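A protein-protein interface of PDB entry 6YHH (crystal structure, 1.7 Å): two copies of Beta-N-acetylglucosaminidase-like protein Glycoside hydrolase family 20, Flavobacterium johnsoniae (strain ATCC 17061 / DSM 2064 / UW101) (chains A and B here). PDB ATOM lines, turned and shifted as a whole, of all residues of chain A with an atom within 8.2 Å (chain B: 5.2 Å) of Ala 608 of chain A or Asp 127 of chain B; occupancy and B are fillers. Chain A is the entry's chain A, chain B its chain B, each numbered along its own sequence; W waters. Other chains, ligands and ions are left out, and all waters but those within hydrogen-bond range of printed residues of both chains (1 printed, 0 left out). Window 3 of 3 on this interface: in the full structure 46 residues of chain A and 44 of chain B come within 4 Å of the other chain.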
ATOM      1  N   ASN A 518      -9.755  16.180  13.155  1.00  0.00           N
ATOM      2  CA  ASN A 518      -9.005  17.256  12.571  1.00  0.00           C
ATOM      3  C   ASN A 518      -9.490  17.549  11.162  1.00  0.00           C
ATOM      4  O   ASN A 518      -8.698  17.858  10.251  1.00  0.00           O
ATOM      5  CB  ASN A 518      -7.496  16.985  12.559  1.00  0.00           C
ATOM      6  CG  ASN A 518      -6.673  18.223  12.383  1.00  0.00           C
ATOM      7  OD1 ASN A 518      -7.138  19.367  12.544  1.00  0.00           O
ATOM      8  ND2 ASN A 518      -5.413  18.020  12.016  1.00  0.00           N
ATOM      9  N   GLN A 520     -10.589  15.803   8.822  1.00  0.00           N
ATOM     10  CA  GLN A 520     -10.436  14.773   7.811  1.00  0.00           C
ATOM     11  C   GLN A 520     -11.769  14.080   7.596  1.00  0.00           C
ATOM     12  O   GLN A 520     -12.804  14.467   8.193  1.00  0.00           O
ATOM     13  CB  GLN A 520      -9.353  13.774   8.270  1.00  0.00           C
ATOM     14  CG  GLN A 520      -7.968  14.396   8.523  1.00  0.00           C
ATOM     15  CD  GLN A 520      -7.020  13.392   9.171  1.00  0.00           C
ATOM     16  OE1 GLN A 520      -6.993  13.188  10.396  1.00  0.00           O
ATOM     17  NE2 GLN A 520      -6.329  12.666   8.328  1.00  0.00           N
ATOM     18  N   GLY A 602      -9.292   2.675   9.056  1.00  0.00           N
ATOM     19  CA  GLY A 602      -9.579   4.059   8.820  1.00  0.00           C
ATOM     20  C   GLY A 602      -9.215   4.960   9.963  1.00  0.00           C
ATOM     21  O   GLY A 602      -8.627   6.050   9.766  1.00  0.00           O
ATOM     22  N   LEU A 603      -9.441   4.478  11.184  1.00  0.00           N
ATOM     23  CA  LEU A 603      -9.066   5.242  12.352  1.00  0.00           C
ATOM     24  C   LEU A 603      -7.544   5.389  12.481  1.00  0.00           C
ATOM     25  O   LEU A 603      -6.985   6.468  12.799  1.00  0.00           O
ATOM     26  CB  LEU A 603      -9.637   4.587  13.590  1.00  0.00           C
ATOM     27  CG  LEU A 603     -11.167   4.611  13.732  1.00  0.00           C
ATOM     28  CD1 LEU A 603     -11.548   3.843  15.013  1.00  0.00           C
ATOM     29  CD2 LEU A 603     -11.643   6.063  13.762  1.00  0.00           C
ATOM     30  N   VAL A 604      -6.837   4.289  12.217  1.00  0.00           N
ATOM     31  CA  VAL A 604      -5.352   4.346  12.240  1.00  0.00           C
ATOM     32  C   VAL A 604      -4.825   5.350  11.194  1.00  0.00           C
ATOM     33  O   VAL A 604      -3.945   6.204  11.508  1.00  0.00           O
ATOM     34  CB  VAL A 604      -4.754   2.936  12.092  1.00  0.00           C
ATOM     35  CG1 VAL A 604      -3.261   2.996  11.849  1.00  0.00           C
ATOM     36  CG2 VAL A 604      -5.049   2.105  13.360  1.00  0.00           C
ATOM     37  N   GLU A 605      -5.411   5.355  10.030  1.00  0.00           N
ATOM     38  CA  GLU A 605      -5.042   6.312   8.958  1.00  0.00           C
ATOM     39  C   GLU A 605      -5.299   7.722   9.499  1.00  0.00           C
ATOM     40  O   GLU A 605      -4.417   8.614   9.392  1.00  0.00           O
ATOM     41  CB  GLU A 605      -5.868   6.147   7.707  1.00  0.00           C
ATOM     42  CG  GLU A 605      -5.679   4.897   6.923  1.00  0.00           C
ATOM     43  CD  GLU A 605      -6.394   5.122   5.574  1.00  0.00           C
ATOM     44  OE1 GLU A 605      -5.843   5.789   4.702  1.00  0.00           O
ATOM     45  OE2 GLU A 605      -7.534   4.722   5.416  1.00  0.00           O
ATOM     46  N   LEU A 606      -6.497   7.970  10.056  1.00  0.00           N
ATOM     47  CA  LEU A 606      -6.794   9.322  10.577  1.00  0.00           C
ATOM     48  C   LEU A 606      -5.869   9.798  11.618  1.00  0.00           C
ATOM     49  O   LEU A 606      -5.512  11.007  11.700  1.00  0.00           O
ATOM     50  CB  LEU A 606      -8.213   9.411  11.160  1.00  0.00           C
ATOM     51  CG  LEU A 606      -9.393   9.262  10.208  1.00  0.00           C
ATOM     52  CD1 LEU A 606     -10.679   9.273  10.988  1.00  0.00           C
ATOM     53  CD2 LEU A 606      -9.363  10.269   9.090  1.00  0.00           C
ATOM     54  N   SER A 607      -5.481   8.858  12.528  1.00  0.00           N
ATOM     55  CA  SER A 607      -4.672   9.206  13.665  1.00  0.00           C
ATOM     56  C   SER A 607      -3.309   9.844  13.391  1.00  0.00           C
ATOM     57  O   SER A 607      -2.812  10.613  14.243  1.00  0.00           O
ATOM     58  CB  SER A 607      -4.506   8.011  14.576  1.00  0.00           C
ATOM     59  OG  SER A 607      -3.506   7.133  14.056  1.00  0.00           O
ATOM     60  N   ALA A 608      -2.782   9.676  12.138  1.00  0.00           N
ATOM     61  CA  ALA A 608      -1.522  10.291  11.769  1.00  0.00           C
ATOM     62  C   ALA A 608      -1.551  11.792  11.916  1.00  0.00           C
ATOM     63  O   ALA A 608      -0.521  12.408  12.182  1.00  0.00           O
ATOM     64  CB  ALA A 608      -1.194   9.870  10.346  1.00  0.00           C
ATOM     65  N   ASN A 609      -2.741  12.371  11.749  1.00  0.00           N
ATOM     66  CA  ASN A 609      -2.911  13.832  11.854  1.00  0.00           C
ATOM     67  C   ASN A 609      -4.071  14.226  12.785  1.00  0.00           C
ATOM     68  O   ASN A 609      -4.724  15.252  12.550  1.00  0.00           O
ATOM     69  CB  ASN A 609      -3.116  14.427  10.467  1.00  0.00           C
ATOM     70  CG  ASN A 609      -3.007  15.983  10.440  1.00  0.00           C
ATOM     71  OD1 ASN A 609      -2.265  16.614  11.219  1.00  0.00           O
ATOM     72  ND2 ASN A 609      -3.720  16.592   9.473  1.00  0.00           N
ATOM     73  N   ALA A 610      -4.315  13.415  13.822  1.00  0.00           N
ATOM     74  CA  ALA A 610      -5.486  13.679  14.697  1.00  0.00           C
ATOM     75  C   ALA A 610      -5.237  13.079  16.097  1.00  0.00           C
ATOM     76  O   ALA A 610      -5.637  11.941  16.346  1.00  0.00           O
ATOM     77  CB  ALA A 610      -6.751  13.099  14.101  1.00  0.00           C
ATOM     78  N   PRO A 611      -4.615  13.842  17.027  1.00  0.00           N
ATOM     79  CA  PRO A 611      -4.383  13.347  18.330  1.00  0.00           C
ATOM     80  C   PRO A 611      -5.638  12.868  19.058  1.00  0.00           C
ATOM     81  O   PRO A 611      -5.514  12.014  19.962  1.00  0.00           O
ATOM     82  CB  PRO A 611      -3.685  14.538  19.064  1.00  0.00           C
ATOM     83  CG  PRO A 611      -3.018  15.299  17.949  1.00  0.00           C
ATOM     84  CD  PRO A 611      -4.021  15.175  16.803  1.00  0.00           C
ATOM     85  N   LEU A 612      -6.805  13.504  18.793  1.00  0.00           N
ATOM     86  CA  LEU A 612      -8.000  13.117  19.527  1.00  0.00           C
ATOM     87  C   LEU A 612      -8.551  11.742  19.094  1.00  0.00           C
ATOM     88  O   LEU A 612      -9.503  11.252  19.679  1.00  0.00           O
ATOM     89  CB  LEU A 612      -9.088  14.180  19.418  1.00  0.00           C
ATOM     90  CG  LEU A 612      -8.700  15.569  19.949  1.00  0.00           C
ATOM     91  CD1 LEU A 612      -9.868  16.484  19.761  1.00  0.00           C
ATOM     92  CD2 LEU A 612      -8.248  15.530  21.330  1.00  0.00           C
ATOM     93  N   VAL A 613      -7.967  11.117  18.071  1.00  0.00           N
ATOM     94  CA  VAL A 613      -8.288   9.740  17.718  1.00  0.00           C
ATOM     95  C   VAL A 613      -7.496   8.731  18.584  1.00  0.00           C
ATOM     96  O   VAL A 613      -7.915   7.608  18.807  1.00  0.00           O
ATOM     97  CB  VAL A 613      -8.082   9.541  16.194  1.00  0.00           C
ATOM     98  CG1 VAL A 613      -8.214   8.064  15.826  1.00  0.00           C
ATOM     99  CG2 VAL A 613      -9.099  10.356  15.374  1.00  0.00           C
ATOM    100  N   GLN A 614      -6.381   9.171  19.158  1.00  0.00           N
ATOM    101  CA  GLN A 614      -5.543   8.277  19.945  1.00  0.00           C
ATOM    102  C   GLN A 614      -6.284   7.559  21.077  1.00  0.00           C
ATOM    103  O   GLN A 614      -6.085   6.382  21.302  1.00  0.00           O
ATOM    104  CB  GLN A 614      -4.318   9.022  20.502  1.00  0.00           C
ATOM    105  CG  GLN A 614      -3.331   9.516  19.431  1.00  0.00           C
ATOM    106  CD  GLN A 614      -2.600   8.387  18.648  1.00  0.00           C
ATOM    107  OE1 GLN A 614      -2.348   7.313  19.187  1.00  0.00           O
ATOM    108  NE2 GLN A 614      -2.200   8.672  17.439  1.00  0.00           N
ATOM    109  N   LEU A 617      -8.130   4.472  19.679  1.00  0.00           N
ATOM    110  CA  LEU A 617      -7.393   3.393  18.949  1.00  0.00           C
ATOM    111  C   LEU A 617      -7.323   2.083  19.727  1.00  0.00           C
ATOM    112  O   LEU A 617      -7.415   0.999  19.134  1.00  0.00           O
ATOM    113  CB  LEU A 617      -5.975   3.887  18.533  1.00  0.00           C
ATOM    114  CG  LEU A 617      -5.939   4.966  17.440  1.00  0.00           C
ATOM    115  CD1 LEU A 617      -4.497   5.236  17.123  1.00  0.00           C
ATOM    116  CD2 LEU A 617      -6.758   4.623  16.186  1.00  0.00           C
ATOM    117  N   GLN B 125      -0.691  23.601  15.847  1.00  0.00           N
ATOM    118  CA  GLN B 125      -0.304  22.501  15.010  1.00  0.00           C
ATOM    119  C   GLN B 125      -0.340  21.206  15.777  1.00  0.00           C
ATOM    120  O   GLN B 125      -0.488  21.185  16.982  1.00  0.00           O
ATOM    121  CB  GLN B 125       1.104  22.730  14.470  1.00  0.00           C
ATOM    122  CG  GLN B 125       1.129  23.827  13.454  1.00  0.00           C
ATOM    123  CD  GLN B 125       2.489  24.253  13.003  1.00  0.00           C
ATOM    124  OE1 GLN B 125       3.499  23.946  13.609  1.00  0.00           O
ATOM    125  NE2 GLN B 125       2.497  25.047  11.955  1.00  0.00           N
ATOM    126  N   ASN B 126      -0.175  20.093  15.072  1.00  0.00           N
ATOM    127  CA  ASN B 126      -0.163  18.837  15.781  1.00  0.00           C
ATOM    128  C   ASN B 126       0.614  17.779  14.992  1.00  0.00           C
ATOM    129  O   ASN B 126       0.808  17.941  13.811  1.00  0.00           O
ATOM    130  CB  ASN B 126      -1.601  18.323  15.988  1.00  0.00           C
ATOM    131  CG  ASN B 126      -2.287  18.053  14.658  1.00  0.00           C
ATOM    132  OD1 ASN B 126      -2.282  16.886  14.140  1.00  0.00           O
ATOM    133  ND2 ASN B 126      -2.781  19.093  14.011  1.00  0.00           N
ATOM    134  N   ASP B 127       1.002  16.744  15.686  1.00  0.00           N
ATOM    135  CA  ASP B 127       1.387  15.465  15.034  1.00  0.00           C
ATOM    136  C   ASP B 127       0.316  14.394  15.273  1.00  0.00           C
ATOM    137  O   ASP B 127      -0.875  14.701  15.352  1.00  0.00           O
ATOM    138  CB  ASP B 127       2.847  15.105  15.408  1.00  0.00           C
ATOM    139  CG  ASP B 127       3.085  14.937  16.831  1.00  0.00           C
ATOM    140  OD1 ASP B 127       2.170  14.691  17.626  1.00  0.00           O
ATOM    141  OD2 ASP B 127       4.251  15.087  17.284  1.00  0.00           O
ATOM    142  N   SER B 128       0.715  13.122  15.359  1.00  0.00           N
ATOM    143  CA  SER B 128      -0.282  12.142  15.646  1.00  0.00           C
ATOM    144  C   SER B 128      -0.758  12.122  17.121  1.00  0.00           C
ATOM    145  O   SER B 128      -1.793  11.508  17.398  1.00  0.00           O
ATOM    146  CB  SER B 128       0.210  10.733  15.226  1.00  0.00           C
ATOM    147  OG  SER B 128       1.271  10.298  16.089  1.00  0.00           O
ATOM    148  N   LYS B 129       0.004  12.743  18.044  1.00  0.00           N
ATOM    149  CA  LYS B 129      -0.211  12.581  19.472  1.00  0.00           C
ATOM    150  C   LYS B 129      -0.310  13.876  20.261  1.00  0.00           C
ATOM    151  O   LYS B 129      -0.952  13.826  21.325  1.00  0.00           O
ATOM    152  CB  LYS B 129       0.905  11.738  20.069  1.00  0.00           C
ATOM    153  CG  LYS B 129       0.671  10.263  19.735  1.00  0.00           C
ATOM    154  CD  LYS B 129       1.904   9.404  20.057  1.00  0.00           C
ATOM    155  CE  LYS B 129       1.576   7.904  20.027  1.00  0.00           C
ATOM    156  N   LYS B 130       0.330  14.932  19.798  1.00  0.00           N
ATOM    157  CA  LYS B 130       0.523  16.144  20.577  1.00  0.00           C
ATOM    158  C   LYS B 130       0.171  17.358  19.761  1.00  0.00           C
ATOM    159  O   LYS B 130       0.201  17.373  18.524  1.00  0.00           O
ATOM    160  CB  LYS B 130       1.986  16.316  21.054  1.00  0.00           C
ATOM    161  N   TYR B 132       1.040  21.613  19.345  1.00  0.00           N
ATOM    162  CA  TYR B 132       2.110  22.545  19.612  1.00  0.00           C
ATOM    163  C   TYR B 132       1.943  23.823  18.791  1.00  0.00           C
ATOM    164  O   TYR B 132       1.131  23.865  17.893  1.00  0.00           O
ATOM    165  CB  TYR B 132       3.460  21.907  19.327  1.00  0.00           C
ATOM    166  CG  TYR B 132       3.577  21.105  18.151  1.00  0.00           C
ATOM    167  CD1 TYR B 132       3.922  21.709  16.913  1.00  0.00           C
ATOM    168  CD2 TYR B 132       3.330  19.764  18.195  1.00  0.00           C
ATOM    169  CE1 TYR B 132       4.086  20.936  15.757  1.00  0.00           C
ATOM    170  CE2 TYR B 132       3.488  18.990  17.078  1.00  0.00           C
ATOM    171  CZ  TYR B 132       3.846  19.574  15.846  1.00  0.00           C
ATOM    172  OH  TYR B 132       3.983  18.804  14.678  1.00  0.00           O
HETATM  173  O   HOH W   1      -3.274  20.249  11.763  1.00  0.00           O
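No position is printed for both chains.
Water W1 bridges the side-chain amide nitrogen (ND2) of Asn 126 of chain B (2.6 Å) and the side-chain amide nitrogen (ND2) of Asn 518 of chain A (3.1 Å).
Of the 16 printed residues of chain A, 7 touch a printed residue of chain B. Hydrophobic or aromatic side chains of chain A within 4 Å of the printed part of chain B: Pro 611. Printed residues of chain B that touch a printed residue of chain A: Asn 126, Asp 127, Ser 128, Lys 129 and Lys 130. Among the printed residues, 13 pairs touch across the chains.
Ala 608 of chain A touches Asp 127 of chain B. Ala 610 of chain A touches Asp 127 of chain B. OD1 of Asn 126 of chain B touches CD of Pro 611 of chain A, at 3.6 Å. Asp 127 of chain B touches Pro 611 of chain A (O to CG, 3.4 Å). CA of Pro 611 of chain A touches O of Ser 128 of chain B, 3.3 Å away. Lys 129 of chain B touches Pro 611 of chain A. N of Lys 130 of chain B touches CG of Pro 611 of chain A, at 3.8 Å. Lys 129 of chain B touches Gln 614 of chain A (CG to CD, 3.9 Å).
The backbone NH (N) of Lys 129 of chain B is in hydrogen-bond range of the side-chain carboxylate (OD1) of Asp 127 of chain B. O of Val 604 of chain A lies within hydrogen-bond range of OG of Ser 607 of chain A, 2.7 Å away. OH of Tyr 132 of chain B lies within hydrogen-bond range of O of Asn 126 of chain B, 3.4 Å away. The backbone NH of Lys 130 of chain B lies within hydrogen-bond range of the side-chain carboxylate of Asp 127 of chain B, at 2.9 Å. ND2 of Asn 518 of chain A lies within hydrogen-bond range of O of Asn 609 of chain A.
The backbone carbonyl oxygen (O) of Ser 607 of chain A lies close to the backbone carbonyl oxygen (O) of Ser 128 of chain B (3.4 Å). ND2 of Asn 518 of chain A lies close to ND2 of Asn 126 of chain B (3.5 Å). The backbone carbonyl oxygen (O) of Ala 608 of chain A sits close to the backbone NH (N) of Ser 128 of chain B (3.5 Å). The side-chain amide oxygen (OD1) of Asn 609 of chain A lies close to the side-chain amide oxygen (OD1) of Asn 126 of chain B, at 2.9 Å. The side-chain amide nitrogen (NE2) of Gln 614 of chain A sits at hydrogen-bond distance from the backbone carbonyl oxygen (O) of Ser 128 of chain B, at 2.9 Å.
Ala 608 of chain A touches just these residues of chain B: Asp 127 and Ser 128. Of the printed residues of chain B, Ala 610 of chain A touches Asp 127 (3.98 Å). Leu 612 of chain A touches none of the printed residues of chain B. Of the printed residues of chain A, Asp 127 of chain B touches Ala 608 (3.8 Å), Ala 610 (3.98 Å) and Pro 611 (3.4 Å). Of the printed residues of chain A, Ser 128 of chain B touches Ser 607 (3.2 Å), Ala 608 (3.5 Å), Pro 611 (3.3 Å) and Gln 614 (2.9 Å). Of the printed residues of chain A, Lys 129 of chain B touches Pro 611 (3.6 Å) and Gln 614 (3.9 Å). Of chain A, only Pro 611 comes within 4 Å of Lys 130 of chain B. Tyr 132 of chain B touches none of the printed residues of chain A. The nearest printed residue of chain B that does not touch Gln 614 of chain A is Asp 127 of chain B (6.5 Å).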
